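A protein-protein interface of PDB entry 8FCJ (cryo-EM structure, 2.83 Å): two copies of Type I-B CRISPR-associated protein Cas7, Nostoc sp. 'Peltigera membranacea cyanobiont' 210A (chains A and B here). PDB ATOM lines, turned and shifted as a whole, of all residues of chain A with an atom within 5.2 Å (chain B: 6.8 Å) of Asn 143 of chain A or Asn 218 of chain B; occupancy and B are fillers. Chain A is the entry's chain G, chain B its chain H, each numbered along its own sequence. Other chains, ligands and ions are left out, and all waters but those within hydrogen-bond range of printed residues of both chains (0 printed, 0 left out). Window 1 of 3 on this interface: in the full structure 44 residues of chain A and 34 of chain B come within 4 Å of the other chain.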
ATOM      1  N   SER A  57      -5.807  11.532 -28.520  1.00  0.00           N
ATOM      2  CA  SER A  57      -5.331  10.846 -27.327  1.00  0.00           C
ATOM      3  C   SER A  57      -4.130   9.960 -27.613  1.00  0.00           C
ATOM      4  O   SER A  57      -3.347   9.684 -26.697  1.00  0.00           O
ATOM      5  CB  SER A  57      -6.457  10.016 -26.716  1.00  0.00           C
ATOM      6  OG  SER A  57      -7.256   9.430 -27.725  1.00  0.00           O
ATOM      7  N   ILE A  60      -1.048  11.834 -26.630  1.00  0.00           N
ATOM      8  CA  ILE A  60      -0.731  11.811 -25.207  1.00  0.00           C
ATOM      9  C   ILE A  60      -0.202  10.443 -24.801  1.00  0.00           C
ATOM     10  O   ILE A  60       0.695  10.334 -23.957  1.00  0.00           O
ATOM     11  CB  ILE A  60      -1.964  12.219 -24.385  1.00  0.00           C
ATOM     12  CG1 ILE A  60      -2.609  13.461 -24.997  1.00  0.00           C
ATOM     13  CG2 ILE A  60      -1.573  12.490 -22.950  1.00  0.00           C
ATOM     14  CD1 ILE A  60      -3.962  13.789 -24.431  1.00  0.00           C
ATOM     15  N   GLY A 141      -6.774   4.187 -20.062  1.00  0.00           N
ATOM     16  CA  GLY A 141      -7.769   4.599 -21.030  1.00  0.00           C
ATOM     17  C   GLY A 141      -7.864   6.106 -21.098  1.00  0.00           C
ATOM     18  O   GLY A 141      -8.154   6.759 -20.092  1.00  0.00           O
ATOM     19  N   MET A 142      -7.622   6.676 -22.274  1.00  0.00           N
ATOM     20  CA  MET A 142      -7.540   8.118 -22.432  1.00  0.00           C
ATOM     21  C   MET A 142      -8.514   8.583 -23.502  1.00  0.00           C
ATOM     22  O   MET A 142      -8.764   7.882 -24.484  1.00  0.00           O
ATOM     23  CB  MET A 142      -6.115   8.555 -22.796  1.00  0.00           C
ATOM     24  CG  MET A 142      -5.902  10.055 -22.785  1.00  0.00           C
ATOM     25  SD  MET A 142      -4.377  10.528 -21.959  1.00  0.00           S
ATOM     26  CE  MET A 142      -3.359   9.095 -22.280  1.00  0.00           C
ATOM     27  N   ASN A 143      -9.068   9.772 -23.295  1.00  0.00           N
ATOM     28  CA  ASN A 143      -9.950  10.415 -24.255  1.00  0.00           C
ATOM     29  C   ASN A 143      -9.235  11.591 -24.907  1.00  0.00           C
ATOM     30  O   ASN A 143      -8.177  12.036 -24.459  1.00  0.00           O
ATOM     31  CB  ASN A 143     -11.246  10.877 -23.584  1.00  0.00           C
ATOM     32  CG  ASN A 143     -12.451  10.728 -24.486  1.00  0.00           C
ATOM     33  OD1 ASN A 143     -12.322  10.674 -25.707  1.00  0.00           O
ATOM     34  ND2 ASN A 143     -13.633  10.651 -23.889  1.00  0.00           N
ATOM     35  N   MET A 144      -9.832  12.089 -25.983  1.00  0.00           N
ATOM     36  CA  MET A 144      -9.209  13.135 -26.778  1.00  0.00           C
ATOM     37  C   MET A 144      -9.090  14.433 -25.986  1.00  0.00           C
ATOM     38  O   MET A 144      -9.925  14.748 -25.136  1.00  0.00           O
ATOM     39  CB  MET A 144     -10.011  13.379 -28.052  1.00  0.00           C
ATOM     40  CG  MET A 144      -9.170  13.795 -29.234  1.00  0.00           C
ATOM     41  SD  MET A 144      -9.784  13.125 -30.782  1.00  0.00           S
ATOM     42  CE  MET A 144     -11.502  13.598 -30.692  1.00  0.00           C
ATOM     43  N   ALA A 145      -8.030  15.184 -26.272  1.00  0.00           N
ATOM     44  CA  ALA A 145      -7.838  16.491 -25.661  1.00  0.00           C
ATOM     45  C   ALA A 145      -8.598  17.543 -26.454  1.00  0.00           C
ATOM     46  O   ALA A 145      -8.447  17.642 -27.673  1.00  0.00           O
ATOM     47  CB  ALA A 145      -6.354  16.842 -25.598  1.00  0.00           C
ATOM     48  N   TYR A 182      -8.136  17.210 -21.206  1.00  0.00           N
ATOM     49  CA  TYR A 182      -8.359  15.835 -21.615  1.00  0.00           C
ATOM     50  C   TYR A 182      -8.689  14.987 -20.399  1.00  0.00           C
ATOM     51  O   TYR A 182      -8.352  15.327 -19.263  1.00  0.00           O
ATOM     52  CB  TYR A 182      -7.153  15.259 -22.368  1.00  0.00           C
ATOM     53  CG  TYR A 182      -5.881  15.141 -21.565  1.00  0.00           C
ATOM     54  CD1 TYR A 182      -5.019  16.217 -21.437  1.00  0.00           C
ATOM     55  CD2 TYR A 182      -5.525  13.943 -20.965  1.00  0.00           C
ATOM     56  CE1 TYR A 182      -3.851  16.111 -20.718  1.00  0.00           C
ATOM     57  CE2 TYR A 182      -4.358  13.828 -20.244  1.00  0.00           C
ATOM     58  CZ  TYR A 182      -3.525  14.915 -20.125  1.00  0.00           C
ATOM     59  OH  TYR A 182      -2.360  14.809 -19.406  1.00  0.00           O
ATOM     60  N   TYR A 183      -9.361  13.873 -20.661  1.00  0.00           N
ATOM     61  CA  TYR A 183      -9.870  12.983 -19.631  1.00  0.00           C
ATOM     62  C   TYR A 183      -9.224  11.617 -19.795  1.00  0.00           C
ATOM     63  O   TYR A 183      -9.162  11.085 -20.907  1.00  0.00           O
ATOM     64  CB  TYR A 183     -11.392  12.876 -19.723  1.00  0.00           C
ATOM     65  CG  TYR A 183     -12.000  11.763 -18.910  1.00  0.00           C
ATOM     66  CD1 TYR A 183     -12.071  11.844 -17.530  1.00  0.00           C
ATOM     67  CD2 TYR A 183     -12.517  10.635 -19.527  1.00  0.00           C
ATOM     68  CE1 TYR A 183     -12.633  10.831 -16.787  1.00  0.00           C
ATOM     69  CE2 TYR A 183     -13.080   9.619 -18.793  1.00  0.00           C
ATOM     70  CZ  TYR A 183     -13.135   9.721 -17.424  1.00  0.00           C
ATOM     71  OH  TYR A 183     -13.698   8.706 -16.691  1.00  0.00           O
ATOM     72  N   PHE A 184      -8.744  11.055 -18.690  1.00  0.00           N
ATOM     73  CA  PHE A 184      -8.097   9.754 -18.697  1.00  0.00           C
ATOM     74  C   PHE A 184      -8.629   8.916 -17.545  1.00  0.00           C
ATOM     75  O   PHE A 184      -9.130   9.436 -16.547  1.00  0.00           O
ATOM     76  CB  PHE A 184      -6.571   9.880 -18.598  1.00  0.00           C
ATOM     77  CG  PHE A 184      -6.085  10.322 -17.249  1.00  0.00           C
ATOM     78  CD1 PHE A 184      -6.046  11.663 -16.922  1.00  0.00           C
ATOM     79  CD2 PHE A 184      -5.661   9.398 -16.312  1.00  0.00           C
ATOM     80  CE1 PHE A 184      -5.599  12.074 -15.685  1.00  0.00           C
ATOM     81  CE2 PHE A 184      -5.216   9.805 -15.075  1.00  0.00           C
ATOM     82  CZ  PHE A 184      -5.185  11.143 -14.763  1.00  0.00           C
ATOM     83  N   GLY A 185      -8.514   7.602 -17.701  1.00  0.00           N
ATOM     84  CA  GLY A 185      -8.910   6.677 -16.662  1.00  0.00           C
ATOM     85  C   GLY A 185      -7.972   5.493 -16.582  1.00  0.00           C
ATOM     86  O   GLY A 185      -7.573   4.944 -17.613  1.00  0.00           O
ATOM     87  N   TYR A 240     -14.137  16.194 -18.372  1.00  0.00           N
ATOM     88  CA  TYR A 240     -14.276  17.515 -18.982  1.00  0.00           C
ATOM     89  C   TYR A 240     -15.076  18.454 -18.080  1.00  0.00           C
ATOM     90  O   TYR A 240     -16.141  18.955 -18.436  1.00  0.00           O
ATOM     91  CB  TYR A 240     -14.908  17.403 -20.371  1.00  0.00           C
ATOM     92  CG  TYR A 240     -14.136  16.516 -21.315  1.00  0.00           C
ATOM     93  CD1 TYR A 240     -12.919  16.921 -21.838  1.00  0.00           C
ATOM     94  CD2 TYR A 240     -14.622  15.271 -21.683  1.00  0.00           C
ATOM     95  CE1 TYR A 240     -12.209  16.115 -22.699  1.00  0.00           C
ATOM     96  CE2 TYR A 240     -13.919  14.458 -22.545  1.00  0.00           C
ATOM     97  CZ  TYR A 240     -12.712  14.886 -23.049  1.00  0.00           C
ATOM     98  OH  TYR A 240     -12.006  14.082 -23.908  1.00  0.00           O
ATOM     99  N   GLY B  25     -19.576  13.477 -24.045  1.00  0.00           N
ATOM    100  CA  GLY B  25     -18.179  13.201 -24.315  1.00  0.00           C
ATOM    101  C   GLY B  25     -18.012  12.661 -25.716  1.00  0.00           C
ATOM    102  O   GLY B  25     -18.986  12.414 -26.434  1.00  0.00           O
ATOM    103  N   LEU B  26     -16.751  12.480 -26.098  1.00  0.00           N
ATOM    104  CA  LEU B  26     -16.426  11.929 -27.404  1.00  0.00           C
ATOM    105  C   LEU B  26     -16.499  10.410 -27.348  1.00  0.00           C
ATOM    106  O   LEU B  26     -15.871   9.784 -26.489  1.00  0.00           O
ATOM    107  CB  LEU B  26     -15.035  12.379 -27.839  1.00  0.00           C
ATOM    108  CG  LEU B  26     -14.820  13.890 -27.877  1.00  0.00           C
ATOM    109  CD1 LEU B  26     -13.529  14.258 -27.174  1.00  0.00           C
ATOM    110  CD2 LEU B  26     -14.815  14.393 -29.302  1.00  0.00           C
ATOM    111  N   ALA B  27     -17.263   9.817 -28.260  1.00  0.00           N
ATOM    112  CA  ALA B  27     -17.531   8.388 -28.226  1.00  0.00           C
ATOM    113  C   ALA B  27     -17.301   7.765 -29.593  1.00  0.00           C
ATOM    114  O   ALA B  27     -17.689   8.328 -30.619  1.00  0.00           O
ATOM    115  CB  ALA B  27     -18.963   8.109 -27.771  1.00  0.00           C
ATOM    116  N   LEU B  29     -17.937   4.119 -29.708  1.00  0.00           N
ATOM    117  CA  LEU B  29     -18.180   2.892 -28.961  1.00  0.00           C
ATOM    118  C   LEU B  29     -18.351   1.650 -29.825  1.00  0.00           C
ATOM    119  O   LEU B  29     -17.522   0.741 -29.766  1.00  0.00           O
ATOM    120  CB  LEU B  29     -19.410   3.072 -28.071  1.00  0.00           C
ATOM    121  CG  LEU B  29     -19.253   4.103 -26.954  1.00  0.00           C
ATOM    122  CD1 LEU B  29     -20.605   4.537 -26.430  1.00  0.00           C
ATOM    123  CD2 LEU B  29     -18.402   3.545 -25.832  1.00  0.00           C
ATOM    124  N   PRO B 208     -19.023  -0.140 -15.979  1.00  0.00           N
ATOM    125  CA  PRO B 208     -17.584   0.097 -16.154  1.00  0.00           C
ATOM    126  C   PRO B 208     -17.252   0.741 -17.487  1.00  0.00           C
ATOM    127  O   PRO B 208     -16.689   1.840 -17.542  1.00  0.00           O
ATOM    128  CB  PRO B 208     -16.977  -1.312 -16.067  1.00  0.00           C
ATOM    129  CG  PRO B 208     -18.104  -2.233 -15.671  1.00  0.00           C
ATOM    130  CD  PRO B 208     -19.365  -1.566 -16.086  1.00  0.00           C
ATOM    131  N   LYS B 209     -17.621   0.059 -18.567  1.00  0.00           N
ATOM    132  CA  LYS B 209     -17.284   0.493 -19.913  1.00  0.00           C
ATOM    133  C   LYS B 209     -18.085  -0.296 -20.937  1.00  0.00           C
ATOM    134  O   LYS B 209     -18.051  -1.530 -20.938  1.00  0.00           O
ATOM    135  CB  LYS B 209     -15.785   0.323 -20.168  1.00  0.00           C
ATOM    136  CG  LYS B 209     -15.350   0.643 -21.582  1.00  0.00           C
ATOM    137  CD  LYS B 209     -14.145  -0.189 -21.987  1.00  0.00           C
ATOM    138  CE  LYS B 209     -14.556  -1.407 -22.790  1.00  0.00           C
ATOM    139  NZ  LYS B 209     -13.406  -1.989 -23.529  1.00  0.00           N
ATOM    140  N   SER B 213     -13.564   1.780 -28.250  1.00  0.00           N
ATOM    141  CA  SER B 213     -12.169   2.193 -28.253  1.00  0.00           C
ATOM    142  C   SER B 213     -11.838   2.989 -26.999  1.00  0.00           C
ATOM    143  O   SER B 213     -11.655   4.207 -27.062  1.00  0.00           O
ATOM    144  CB  SER B 213     -11.859   3.020 -29.500  1.00  0.00           C
ATOM    145  OG  SER B 213     -12.351   2.382 -30.662  1.00  0.00           O
ATOM    146  N   SER B 214     -11.754   2.307 -25.856  1.00  0.00           N
ATOM    147  CA  SER B 214     -11.419   2.985 -24.611  1.00  0.00           C
ATOM    148  C   SER B 214      -9.991   3.506 -24.602  1.00  0.00           C
ATOM    149  O   SER B 214      -9.681   4.410 -23.822  1.00  0.00           O
ATOM    150  CB  SER B 214     -11.633   2.045 -23.428  1.00  0.00           C
ATOM    151  OG  SER B 214     -10.482   1.253 -23.201  1.00  0.00           O
ATOM    152  N   ASN B 215      -9.114   2.952 -25.440  1.00  0.00           N
ATOM    153  CA  ASN B 215      -7.746   3.450 -25.508  1.00  0.00           C
ATOM    154  C   ASN B 215      -7.700   4.863 -26.072  1.00  0.00           C
ATOM    155  O   ASN B 215      -6.942   5.709 -25.585  1.00  0.00           O
ATOM    156  CB  ASN B 215      -6.886   2.510 -26.349  1.00  0.00           C
ATOM    157  CG  ASN B 215      -7.410   2.348 -27.758  1.00  0.00           C
ATOM    158  OD1 ASN B 215      -8.616   2.369 -27.988  1.00  0.00           O
ATOM    159  ND2 ASN B 215      -6.504   2.184 -28.711  1.00  0.00           N
ATOM    160  N   ILE B 216      -8.503   5.138 -27.094  1.00  0.00           N
ATOM    161  CA  ILE B 216      -8.483   6.421 -27.778  1.00  0.00           C
ATOM    162  C   ILE B 216      -9.652   7.301 -27.358  1.00  0.00           C
ATOM    163  O   ILE B 216      -9.483   8.503 -27.152  1.00  0.00           O
ATOM    164  CB  ILE B 216      -8.466   6.204 -29.306  1.00  0.00           C
ATOM    165  CG1 ILE B 216      -7.178   5.505 -29.730  1.00  0.00           C
ATOM    166  CG2 ILE B 216      -8.573   7.524 -30.033  1.00  0.00           C
ATOM    167  CD1 ILE B 216      -5.940   6.020 -29.030  1.00  0.00           C
ATOM    168  N   PHE B 217     -10.841   6.721 -27.219  1.00  0.00           N
ATOM    169  CA  PHE B 217     -12.043   7.450 -26.821  1.00  0.00           C
ATOM    170  C   PHE B 217     -12.605   6.794 -25.566  1.00  0.00           C
ATOM    171  O   PHE B 217     -13.479   5.929 -25.644  1.00  0.00           O
ATOM    172  CB  PHE B 217     -13.072   7.459 -27.940  1.00  0.00           C
ATOM    173  CG  PHE B 217     -12.597   8.119 -29.197  1.00  0.00           C
ATOM    174  CD1 PHE B 217     -12.597   9.496 -29.313  1.00  0.00           C
ATOM    175  CD2 PHE B 217     -12.158   7.364 -30.266  1.00  0.00           C
ATOM    176  CE1 PHE B 217     -12.164  10.103 -30.470  1.00  0.00           C
ATOM    177  CE2 PHE B 217     -11.727   7.968 -31.427  1.00  0.00           C
ATOM    178  CZ  PHE B 217     -11.728   9.338 -31.527  1.00  0.00           C
ATOM    179  N   ASN B 218     -12.111   7.215 -24.406  1.00  0.00           N
ATOM    180  CA  ASN B 218     -12.605   6.701 -23.133  1.00  0.00           C
ATOM    181  C   ASN B 218     -13.914   7.404 -22.803  1.00  0.00           C
ATOM    182  O   ASN B 218     -13.918   8.583 -22.436  1.00  0.00           O
ATOM    183  CB  ASN B 218     -11.571   6.912 -22.033  1.00  0.00           C
ATOM    184  CG  ASN B 218     -11.901   6.144 -20.773  1.00  0.00           C
ATOM    185  OD1 ASN B 218     -12.811   5.319 -20.757  1.00  0.00           O
ATOM    186  ND2 ASN B 218     -11.159   6.411 -19.707  1.00  0.00           N
ATOM    187  N   TYR B 219     -15.025   6.688 -22.936  1.00  0.00           N
ATOM    188  CA  TYR B 219     -16.358   7.256 -22.740  1.00  0.00           C
ATOM    189  C   TYR B 219     -17.037   6.578 -21.562  1.00  0.00           C
ATOM    190  O   TYR B 219     -17.524   5.441 -21.694  1.00  0.00           O
ATOM    191  CB  TYR B 219     -17.196   7.094 -24.007  1.00  0.00           C
ATOM    192  CG  TYR B 219     -18.510   7.836 -23.982  1.00  0.00           C
ATOM    193  CD1 TYR B 219     -18.593   9.153 -24.403  1.00  0.00           C
ATOM    194  CD2 TYR B 219     -19.670   7.215 -23.549  1.00  0.00           C
ATOM    195  CE1 TYR B 219     -19.790   9.831 -24.388  1.00  0.00           C
ATOM    196  CE2 TYR B 219     -20.872   7.886 -23.530  1.00  0.00           C
ATOM    197  CZ  TYR B 219     -20.926   9.193 -23.950  1.00  0.00           C
ATOM    198  OH  TYR B 219     -22.122   9.867 -23.932  1.00  0.00           O
ATOM    199  N   PRO B 220     -17.095   7.219 -20.396  1.00  0.00           N
ATOM    200  CA  PRO B 220     -17.798   6.612 -19.259  1.00  0.00           C
ATOM    201  C   PRO B 220     -19.292   6.528 -19.531  1.00  0.00           C
ATOM    202  O   PRO B 220     -19.916   7.500 -19.958  1.00  0.00           O
ATOM    203  CB  PRO B 220     -17.488   7.563 -18.099  1.00  0.00           C
ATOM    204  CG  PRO B 220     -17.176   8.862 -18.753  1.00  0.00           C
ATOM    205  CD  PRO B 220     -16.513   8.526 -20.054  1.00  0.00           C
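The backbone carbonyl oxygen (O) of Gly 141 of chain A lies within hydrogen-bond range of the backbone NH (N) of Gly 185 of chain A (2.6 Å).
O of Tyr 183 of chain A sits at hydrogen-bond distance from N of Asn 143 of chain A.
The backbone carbonyl oxygen of Met 144 of chain A lies within hydrogen-bond range of the side-chain hydroxyl of Tyr 240 of chain A (2.5 Å).
Printed residues of chain B within 4 Å of Ser 57 of chain A: Ile 216.
Of the printed residues of chain B, Met 142 of chain A touches Ser 214, Asn 215, Ile 216, Phe 217 and Asn 218.
Of chain B, only Leu 26, Ile 216, Phe 217 and Asn 218 come within 4 Å of Asn 143 of chain A.
Of the printed residues of chain A, Leu 26 of chain B touches Asn 143 (3.5 Å), Met 144 (3.7 Å) and Tyr 240 (3.6 Å).
Of the printed residues of chain A, Ser 214 of chain B touches Gly 141 and Met 142.
The nearest residue of chain B that does not touch Asn 143 of chain A is Tyr 219 of chain B (4.3 Å).
The nearest printed residue of chain B that does not touch Tyr 240 of chain A is Gly 25 of chain B (4.8 Å).
Among the printed residues, pairs that only touch across the chains: Gly 141 of chain A with Ser 214 of chain B (3.4 Å), Met 142 of chain A with Phe 217 of chain B (3.6 Å), Asn 143 of chain A with Leu 26 of chain B (3.5 Å), Asn 143 of chain A with Ile 216 of chain B (3.5 Å), Asn 143 of chain A with Phe 217 of chain B (3.4 Å), Met 144 of chain A with Leu 26 of chain B (3.7 Å), Met 144 of chain A with Ile 216 of chain B (3.8 Å), Met 144 of chain A with Phe 217 of chain B (3.6 Å), Tyr 183 of chain A with Asn 218 of chain B (3.8 Å), Tyr 183 of chain A with Pro 220 of chain B (3.8 Å), Gly 185 of chain A with Asn 218 of chain B (3.5 Å) and Tyr 240 of chain A with Leu 26 of chain B (3.6 Å).
No position is printed for both chains.
Of the 14 printed residues of chain B, 7 touch a printed residue of chain A.
Printed residues of chain B that touch a printed residue of chain A: Leu 26, Ser 214, Asn 215, Ile 216, Phe 217, Asn 218 and Pro 220.
Hydrophobic or aromatic side chains of chain B that line the printed part of chain A: Leu 26, Ile 216, Phe 217 and Pro 220.
Of the 12 printed residues of chain A, 8 touch a printed residue of chain B.
Printed residues of chain A that touch a printed residue of chain B: Ser 57, Gly 141, Met 142, Asn 143, Met 144, Tyr 183, Gly 185 and Tyr 240.
Among the printed residues, no Asp or Glu carboxylate lies within 4 Å of a Lys or Arg side-chain nitrogen of the other chain.
The backbone carbonyl oxygen (O) of Ile 216 of chain B sits at hydrogen-bond distance from the side-chain hydroxyl (OG) of Ser 57 of chain A.
The backbone carbonyl oxygen (O) of Gly 141 of chain A is in hydrogen-bond range of the side-chain amide nitrogen (ND2) of Asn 218 of chain B (3.0 Å).
O of Ser 214 of chain B sits at hydrogen-bond distance from N of Met 142 of chain A, 3.4 Å away.
The backbone carbonyl oxygen (O) of Met 142 of chain A sits at hydrogen-bond distance from the backbone NH (N) of Asn 218 of chain B, 3.4 Å away.
ND2 of Asn 143 of chain A lies within hydrogen-bond range of O of Asn 218 of chain B, 2.5 Å away.
The backbone carbonyl oxygen of Asn 215 of chain B lies close to the backbone carbonyl oxygen of Met 142 of chain A (3.0 Å).
The backbone carbonyl oxygen (O) of Met 142 of chain A lies close to the backbone carbonyl oxygen (O) of Ile 216 of chain B (2.8 Å).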
